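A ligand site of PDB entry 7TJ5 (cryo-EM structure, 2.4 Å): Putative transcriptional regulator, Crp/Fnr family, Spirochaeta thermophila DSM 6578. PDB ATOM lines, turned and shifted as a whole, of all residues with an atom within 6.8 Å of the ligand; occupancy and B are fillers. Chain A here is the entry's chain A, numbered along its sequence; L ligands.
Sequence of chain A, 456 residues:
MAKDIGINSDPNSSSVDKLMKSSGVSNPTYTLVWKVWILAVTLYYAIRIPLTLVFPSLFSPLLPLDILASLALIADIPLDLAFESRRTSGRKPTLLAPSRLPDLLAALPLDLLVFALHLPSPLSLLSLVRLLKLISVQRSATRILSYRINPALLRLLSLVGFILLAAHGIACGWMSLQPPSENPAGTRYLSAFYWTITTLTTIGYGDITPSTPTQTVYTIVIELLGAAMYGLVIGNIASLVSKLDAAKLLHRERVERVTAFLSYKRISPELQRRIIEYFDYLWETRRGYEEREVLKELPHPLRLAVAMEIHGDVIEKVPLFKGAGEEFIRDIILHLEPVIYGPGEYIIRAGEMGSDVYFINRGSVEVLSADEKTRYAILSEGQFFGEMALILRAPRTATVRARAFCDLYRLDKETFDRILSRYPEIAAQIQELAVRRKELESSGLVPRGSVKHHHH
N of Gly 386 lies within hydrogen-bond range of O6 of the ligand (2.5 Å). An oxygen (O3) of the ligand sits at hydrogen-bond distance from the side-chain hydroxyl of Thr 397. The backbone NH (N) of Thr 397 sits at hydrogen-bond distance from an oxygen (O3) of the ligand (2.9 Å). The side-chain carboxylate (OE1) of Glu 387 is in hydrogen-bond range of an oxygen (O6) of the ligand (3.0 Å). An oxygen (O2) of the ligand is in salt-bridge range of the guanidinium group (NH1) of Arg 396, at 2.9 Å.
The backbone NH (N) of Phe 385 sits at hydrogen-bond distance from the backbone carbonyl oxygen (O) of Tyr 358 (3.1 Å). The backbone NH (N) of Tyr 376 lies within hydrogen-bond range of the backbone carbonyl oxygen (O) of Val 367, at 2.9 Å. The backbone carbonyl oxygen (O) of Ile 348 is in hydrogen-bond range of the backbone NH (N) of Val 400, at 2.8 Å. The guanidinium group of Arg 396 is in hydrogen-bond range of the backbone carbonyl oxygen of Asp 356.
Residues that only touch the ligand: Ile 348 (3.4 Å), Tyr 376 (3.9 Å), Phe 385 (3.3 Å), Met 388 (3.2 Å) and Ala 398 (3.3 Å). Hydrophobic or aromatic side chains that line the ligand: Ile 348, Tyr 376, Phe 385, Met 388 and Ala 398. Along chain A the residues within 4 Å of the ligand span positions 348 to 398. The nearest printed residue that does not touch the ligand is Ala 377 (4.03 Å).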
ATOM      1  N   ILE A 348      25.799  -3.869  27.960  1.00  0.00           N
ATOM      2  CA  ILE A 348      25.121  -2.584  27.622  1.00  0.00           C
ATOM      3  C   ILE A 348      23.630  -2.874  27.701  1.00  0.00           C
ATOM      4  O   ILE A 348      23.206  -3.897  27.181  1.00  0.00           O
ATOM      5  CB  ILE A 348      25.505  -2.124  26.206  1.00  0.00           C
ATOM      6  CG1 ILE A 348      27.002  -1.865  26.053  1.00  0.00           C
ATOM      7  CG2 ILE A 348      24.680  -0.923  25.779  1.00  0.00           C
ATOM      8  CD1 ILE A 348      27.410  -1.443  24.660  1.00  0.00           C
ATOM      9  N   ARG A 349      22.865  -1.989  28.354  1.00  0.00           N
ATOM     10  CA  ARG A 349      21.396  -2.174  28.414  1.00  0.00           C
ATOM     11  C   ARG A 349      20.715  -1.181  27.483  1.00  0.00           C
ATOM     12  O   ARG A 349      21.183  -0.039  27.404  1.00  0.00           O
ATOM     13  CB  ARG A 349      20.876  -2.119  29.854  1.00  0.00           C
ATOM     14  CG  ARG A 349      21.322  -3.264  30.749  1.00  0.00           C
ATOM     15  CD  ARG A 349      20.718  -3.127  32.130  1.00  0.00           C
ATOM     16  NE  ARG A 349      21.179  -4.173  33.027  1.00  0.00           N
ATOM     17  CZ  ARG A 349      20.891  -4.232  34.326  1.00  0.00           C
ATOM     18  NH1 ARG A 349      20.147  -3.293  34.874  1.00  0.00           N
ATOM     19  NH2 ARG A 349      21.362  -5.219  35.061  1.00  0.00           N
ATOM     20  N   MET A 353      22.115   5.846  28.928  1.00  0.00           N
ATOM     21  CA  MET A 353      22.932   6.869  28.290  1.00  0.00           C
ATOM     22  C   MET A 353      24.152   6.248  27.633  1.00  0.00           C
ATOM     23  O   MET A 353      24.253   6.220  26.401  1.00  0.00           O
ATOM     24  CB  MET A 353      23.337   7.930  29.321  1.00  0.00           C
ATOM     25  CG  MET A 353      24.083   9.117  28.748  1.00  0.00           C
ATOM     26  SD  MET A 353      24.108  10.484  29.906  1.00  0.00           S
ATOM     27  CE  MET A 353      25.741  11.139  29.615  1.00  0.00           C
ATOM     28  N   GLY A 354      25.081   5.733  28.433  1.00  0.00           N
ATOM     29  CA  GLY A 354      26.256   5.059  27.902  1.00  0.00           C
ATOM     30  C   GLY A 354      27.452   5.935  27.622  1.00  0.00           C
ATOM     31  O   GLY A 354      27.326   7.014  27.030  1.00  0.00           O
ATOM     32  N   ASP A 356      30.942   4.182  27.269  1.00  0.00           N
ATOM     33  CA  ASP A 356      32.105   3.321  27.107  1.00  0.00           C
ATOM     34  C   ASP A 356      32.011   2.554  25.793  1.00  0.00           C
ATOM     35  O   ASP A 356      30.935   2.348  25.241  1.00  0.00           O
ATOM     36  CB  ASP A 356      32.255   2.326  28.276  1.00  0.00           C
ATOM     37  CG  ASP A 356      32.466   3.023  29.619  1.00  0.00           C
ATOM     38  OD1 ASP A 356      31.784   4.019  29.906  1.00  0.00           O
ATOM     39  OD2 ASP A 356      33.290   2.536  30.417  1.00  0.00           O
ATOM     40  N   TYR A 358      33.638  -1.138  23.954  1.00  0.00           N
ATOM     41  CA  TYR A 358      34.116  -2.460  24.352  1.00  0.00           C
ATOM     42  C   TYR A 358      34.725  -3.174  23.153  1.00  0.00           C
ATOM     43  O   TYR A 358      34.137  -3.181  22.065  1.00  0.00           O
ATOM     44  CB  TYR A 358      32.988  -3.317  24.926  1.00  0.00           C
ATOM     45  CG  TYR A 358      32.321  -2.740  26.152  1.00  0.00           C
ATOM     46  CD1 TYR A 358      32.876  -2.881  27.406  1.00  0.00           C
ATOM     47  CD2 TYR A 358      31.097  -2.081  26.050  1.00  0.00           C
ATOM     48  CE1 TYR A 358      32.261  -2.380  28.523  1.00  0.00           C
ATOM     49  CE2 TYR A 358      30.473  -1.569  27.172  1.00  0.00           C
ATOM     50  CZ  TYR A 358      31.060  -1.720  28.401  1.00  0.00           C
ATOM     51  OH  TYR A 358      30.447  -1.213  29.531  1.00  0.00           O
ATOM     52  N   VAL A 367      23.886  -9.561  20.531  1.00  0.00           N
ATOM     53  CA  VAL A 367      23.181  -8.285  20.480  1.00  0.00           C
ATOM     54  C   VAL A 367      21.684  -8.579  20.375  1.00  0.00           C
ATOM     55  O   VAL A 367      21.267  -9.399  19.552  1.00  0.00           O
ATOM     56  CB  VAL A 367      23.678  -7.433  19.297  1.00  0.00           C
ATOM     57  CG1 VAL A 367      22.953  -6.091  19.279  1.00  0.00           C
ATOM     58  CG2 VAL A 367      25.176  -7.222  19.396  1.00  0.00           C
ATOM     59  N   TYR A 376      19.933  -9.466  16.924  1.00  0.00           N
ATOM     60  CA  TYR A 376      20.543  -8.719  15.823  1.00  0.00           C
ATOM     61  C   TYR A 376      21.785  -9.408  15.279  1.00  0.00           C
ATOM     62  O   TYR A 376      21.933  -9.572  14.069  1.00  0.00           O
ATOM     63  CB  TYR A 376      20.877  -7.285  16.250  1.00  0.00           C
ATOM     64  CG  TYR A 376      19.720  -6.407  16.677  1.00  0.00           C
ATOM     65  CD1 TYR A 376      18.879  -6.754  17.727  1.00  0.00           C
ATOM     66  CD2 TYR A 376      19.486  -5.194  16.036  1.00  0.00           C
ATOM     67  CE1 TYR A 376      17.832  -5.943  18.095  1.00  0.00           C
ATOM     68  CE2 TYR A 376      18.444  -4.370  16.403  1.00  0.00           C
ATOM     69  CZ  TYR A 376      17.620  -4.753  17.436  1.00  0.00           C
ATOM     70  OH  TYR A 376      16.576  -3.935  17.816  1.00  0.00           O
ATOM     71  N   ALA A 377      22.684  -9.840  16.162  1.00  0.00           N
ATOM     72  CA  ALA A 377      23.959 -10.384  15.706  1.00  0.00           C
ATOM     73  C   ALA A 377      24.646 -11.120  16.841  1.00  0.00           C
ATOM     74  O   ALA A 377      24.282 -10.995  18.017  1.00  0.00           O
ATOM     75  CB  ALA A 377      24.871  -9.282  15.161  1.00  0.00           C
ATOM     76  N   ILE A 378      25.657 -11.889  16.467  1.00  0.00           N
ATOM     77  CA  ILE A 378      26.537 -12.599  17.395  1.00  0.00           C
ATOM     78  C   ILE A 378      27.957 -12.126  17.112  1.00  0.00           C
ATOM     79  O   ILE A 378      28.421 -12.188  15.963  1.00  0.00           O
ATOM     80  CB  ILE A 378      26.424 -14.118  17.236  1.00  0.00           C
ATOM     81  CG1 ILE A 378      25.046 -14.606  17.681  1.00  0.00           C
ATOM     82  CG2 ILE A 378      27.534 -14.821  18.009  1.00  0.00           C
ATOM     83  CD1 ILE A 378      24.705 -16.002  17.219  1.00  0.00           C
ATOM     84  N   LEU A 379      28.634 -11.634  18.145  1.00  0.00           N
ATOM     85  CA  LEU A 379      29.974 -11.084  18.000  1.00  0.00           C
ATOM     86  C   LEU A 379      31.007 -12.006  18.636  1.00  0.00           C
ATOM     87  O   LEU A 379      30.802 -12.546  19.725  1.00  0.00           O
ATOM     88  CB  LEU A 379      30.062  -9.688  18.626  1.00  0.00           C
ATOM     89  CG  LEU A 379      28.998  -8.676  18.217  1.00  0.00           C
ATOM     90  CD1 LEU A 379      29.374  -7.286  18.716  1.00  0.00           C
ATOM     91  CD2 LEU A 379      28.829  -8.655  16.706  1.00  0.00           C
ATOM     92  N   PHE A 384      33.987  -5.473  17.905  1.00  0.00           N
ATOM     93  CA  PHE A 384      33.724  -4.478  18.943  1.00  0.00           C
ATOM     94  C   PHE A 384      32.279  -4.042  18.866  1.00  0.00           C
ATOM     95  O   PHE A 384      31.575  -4.310  17.890  1.00  0.00           O
ATOM     96  CB  PHE A 384      34.728  -3.300  18.827  1.00  0.00           C
ATOM     97  CG  PHE A 384      34.593  -2.487  17.548  1.00  0.00           C
ATOM     98  CD1 PHE A 384      33.483  -1.677  17.296  1.00  0.00           C
ATOM     99  CD2 PHE A 384      35.574  -2.583  16.582  1.00  0.00           C
ATOM    100  CE1 PHE A 384      33.393  -0.955  16.113  1.00  0.00           C
ATOM    101  CE2 PHE A 384      35.477  -1.866  15.395  1.00  0.00           C
ATOM    102  CZ  PHE A 384      34.391  -1.057  15.170  1.00  0.00           C
ATOM    103  N   PHE A 385      31.829  -3.372  19.935  1.00  0.00           N
ATOM    104  CA  PHE A 385      30.482  -2.815  19.968  1.00  0.00           C
ATOM    105  C   PHE A 385      30.497  -1.583  20.858  1.00  0.00           C
ATOM    106  O   PHE A 385      31.388  -1.400  21.695  1.00  0.00           O
ATOM    107  CB  PHE A 385      29.447  -3.822  20.464  1.00  0.00           C
ATOM    108  CG  PHE A 385      29.832  -4.525  21.748  1.00  0.00           C
ATOM    109  CD1 PHE A 385      30.577  -5.694  21.719  1.00  0.00           C
ATOM    110  CD2 PHE A 385      29.429  -4.015  22.964  1.00  0.00           C
ATOM    111  CE1 PHE A 385      30.931  -6.318  22.894  1.00  0.00           C
ATOM    112  CE2 PHE A 385      29.770  -4.642  24.144  1.00  0.00           C
ATOM    113  CZ  PHE A 385      30.525  -5.799  24.107  1.00  0.00           C
ATOM    114  N   GLY A 386      29.487  -0.734  20.686  1.00  0.00           N
ATOM    115  CA  GLY A 386      29.436   0.514  21.411  1.00  0.00           C
ATOM    116  C   GLY A 386      30.295   1.604  20.834  1.00  0.00           C
ATOM    117  O   GLY A 386      30.678   2.527  21.553  1.00  0.00           O
ATOM    118  N   GLU A 387      30.624   1.530  19.540  1.00  0.00           N
ATOM    119  CA  GLU A 387      31.493   2.527  18.929  1.00  0.00           C
ATOM    120  C   GLU A 387      30.809   3.871  18.780  1.00  0.00           C
ATOM    121  O   GLU A 387      31.487   4.897  18.679  1.00  0.00           O
ATOM    122  CB  GLU A 387      32.000   2.027  17.572  1.00  0.00           C
ATOM    123  CG  GLU A 387      30.930   1.945  16.491  1.00  0.00           C
ATOM    124  CD  GLU A 387      30.278   0.575  16.427  1.00  0.00           C
ATOM    125  OE1 GLU A 387      29.973   0.010  17.493  1.00  0.00           O
ATOM    126  OE2 GLU A 387      30.077   0.073  15.303  1.00  0.00           O
ATOM    127  N   MET A 388      29.476   3.895  18.751  1.00  0.00           N
ATOM    128  CA  MET A 388      28.727   5.156  18.627  1.00  0.00           C
ATOM    129  C   MET A 388      28.437   5.754  19.993  1.00  0.00           C
ATOM    130  O   MET A 388      27.313   6.121  20.318  1.00  0.00           O
ATOM    131  CB  MET A 388      27.456   4.928  17.833  1.00  0.00           C
ATOM    132  CG  MET A 388      26.754   3.617  18.121  1.00  0.00           C
ATOM    133  SD  MET A 388      25.298   3.365  17.093  1.00  0.00           S
ATOM    134  CE  MET A 388      26.048   2.860  15.544  1.00  0.00           C
ATOM    135  N   ALA A 389      29.481   5.848  20.814  1.00  0.00           N
ATOM    136  CA  ALA A 389      29.411   6.529  22.100  1.00  0.00           C
ATOM    137  C   ALA A 389      30.596   7.440  22.372  1.00  0.00           C
ATOM    138  O   ALA A 389      30.513   8.272  23.282  1.00  0.00           O
ATOM    139  CB  ALA A 389      29.296   5.526  23.245  1.00  0.00           C
ATOM    140  N   ALA A 394      24.427   9.823  23.168  1.00  0.00           N
ATOM    141  CA  ALA A 394      23.035   9.526  22.889  1.00  0.00           C
ATOM    142  C   ALA A 394      22.592   8.265  23.635  1.00  0.00           C
ATOM    143  O   ALA A 394      23.438   7.490  24.085  1.00  0.00           O
ATOM    144  CB  ALA A 394      22.870   9.375  21.379  1.00  0.00           C
ATOM    145  N   PRO A 395      21.278   8.027  23.781  1.00  0.00           N
ATOM    146  CA  PRO A 395      20.836   6.730  24.319  1.00  0.00           C
ATOM    147  C   PRO A 395      21.272   5.570  23.438  1.00  0.00           C
ATOM    148  O   PRO A 395      21.388   5.693  22.221  1.00  0.00           O
ATOM    149  CB  PRO A 395      19.307   6.871  24.381  1.00  0.00           C
ATOM    150  CG  PRO A 395      19.012   8.288  23.961  1.00  0.00           C
ATOM    151  CD  PRO A 395      20.144   8.722  23.140  1.00  0.00           C
ATOM    152  N   ARG A 396      21.518   4.428  24.072  1.00  0.00           N
ATOM    153  CA  ARG A 396      22.079   3.284  23.377  1.00  0.00           C
ATOM    154  C   ARG A 396      21.025   2.679  22.438  1.00  0.00           C
ATOM    155  O   ARG A 396      19.816   2.914  22.590  1.00  0.00           O
ATOM    156  CB  ARG A 396      22.559   2.231  24.372  1.00  0.00           C
ATOM    157  CG  ARG A 396      23.600   2.758  25.354  1.00  0.00           C
ATOM    158  CD  ARG A 396      25.000   2.778  24.778  1.00  0.00           C
ATOM    159  NE  ARG A 396      25.990   2.389  25.783  1.00  0.00           N
ATOM    160  CZ  ARG A 396      27.301   2.404  25.585  1.00  0.00           C
ATOM    161  NH1 ARG A 396      27.820   2.779  24.430  1.00  0.00           N
ATOM    162  NH2 ARG A 396      28.107   2.033  26.577  1.00  0.00           N
ATOM    163  N   THR A 397      21.485   1.886  21.473  1.00  0.00           N
ATOM    164  CA  THR A 397      20.607   1.380  20.423  1.00  0.00           C
ATOM    165  C   THR A 397      20.309  -0.110  20.513  1.00  0.00           C
ATOM    166  O   THR A 397      19.517  -0.596  19.694  1.00  0.00           O
ATOM    167  CB  THR A 397      21.199   1.695  19.049  1.00  0.00           C
ATOM    168  OG1 THR A 397      22.283   0.788  18.774  1.00  0.00           O
ATOM    169  CG2 THR A 397      21.721   3.124  18.995  1.00  0.00           C
ATOM    170  N   ALA A 398      20.866  -0.838  21.467  1.00  0.00           N
ATOM    171  CA  ALA A 398      20.546  -2.254  21.637  1.00  0.00           C
ATOM    172  C   ALA A 398      21.089  -2.743  22.979  1.00  0.00           C
ATOM    173  O   ALA A 398      21.762  -2.007  23.706  1.00  0.00           O
ATOM    174  CB  ALA A 398      21.116  -3.106  20.501  1.00  0.00           C
ATOM    175  N   THR A 399      20.779  -3.992  23.278  1.00  0.00           N
ATOM    176  CA  THR A 399      21.156  -4.662  24.513  1.00  0.00           C
ATOM    177  C   THR A 399      22.254  -5.686  24.199  1.00  0.00           C
ATOM    178  O   THR A 399      22.159  -6.404  23.200  1.00  0.00           O
ATOM    179  CB  THR A 399      19.962  -5.357  25.168  1.00  0.00           C
ATOM    180  OG1 THR A 399      18.991  -4.377  25.561  1.00  0.00           O
ATOM    181  CG2 THR A 399      20.380  -6.138  26.405  1.00  0.00           C
ATOM    182  N   VAL A 400      23.294  -5.731  25.021  1.00  0.00           N
ATOM    183  CA  VAL A 400      24.430  -6.611  24.786  1.00  0.00           C
ATOM    184  C   VAL A 400      24.510  -7.613  25.923  1.00  0.00           C
ATOM    185  O   VAL A 400      24.560  -7.218  27.093  1.00  0.00           O
ATOM    186  CB  VAL A 400      25.738  -5.812  24.653  1.00  0.00           C
ATOM    187  CG1 VAL A 400      26.908  -6.728  24.568  1.00  0.00           C
ATOM    188  CG2 VAL A 400      25.681  -4.951  23.391  1.00  0.00           C
HETATM  189  P1  LIG L   1      25.629   1.573  21.341  1.00  0.00           P
HETATM  190  O1  LIG L   1      25.357   3.054  21.224  1.00  0.00           O
HETATM  191  O2  LIG L   1      26.493   1.054  22.473  1.00  0.00           O
HETATM  192  O3  LIG L   1      24.225   0.813  21.488  1.00  0.00           O
HETATM  193  C1  LIG L   1      24.165  -0.614  21.490  1.00  0.00           C
HETATM  194  C2  LIG L   1      25.253  -1.120  20.580  1.00  0.00           C
HETATM  195  O4  LIG L   1      24.882  -2.338  19.892  1.00  0.00           O
HETATM  196  C3  LIG L   1      25.574  -0.179  19.459  1.00  0.00           C
HETATM  197  O5  LIG L   1      26.204   1.007  19.933  1.00  0.00           O
HETATM  198  C4  LIG L   1      26.375  -1.065  18.515  1.00  0.00           C
HETATM  199  O6  LIG L   1      27.706  -1.235  18.994  1.00  0.00           O
HETATM  200  C5  LIG L   1      25.624  -2.403  18.681  1.00  0.00           C
HETATM  201  N1  LIG L   1      24.689  -2.658  17.566  1.00  0.00           N
HETATM  202  C6  LIG L   1      23.533  -2.005  17.341  1.00  0.00           C
HETATM  203  N2  LIG L   1      22.913  -2.486  16.233  1.00  0.00           N
HETATM  204  C7  LIG L   1      23.676  -3.476  15.733  1.00  0.00           C
HETATM  205  C8  LIG L   1      23.606  -4.403  14.587  1.00  0.00           C
HETATM  206  N3  LIG L   1      22.555  -4.368  13.725  1.00  0.00           N
HETATM  207  N4  LIG L   1      24.615  -5.285  14.428  1.00  0.00           N
HETATM  208  C9  LIG L   1      25.655  -5.332  15.274  1.00  0.00           C
HETATM  209  N5  LIG L   1      25.788  -4.522  16.339  1.00  0.00           N
HETATM  210  C10 LIG L   1      24.844  -3.581  16.625  1.00  0.00           C
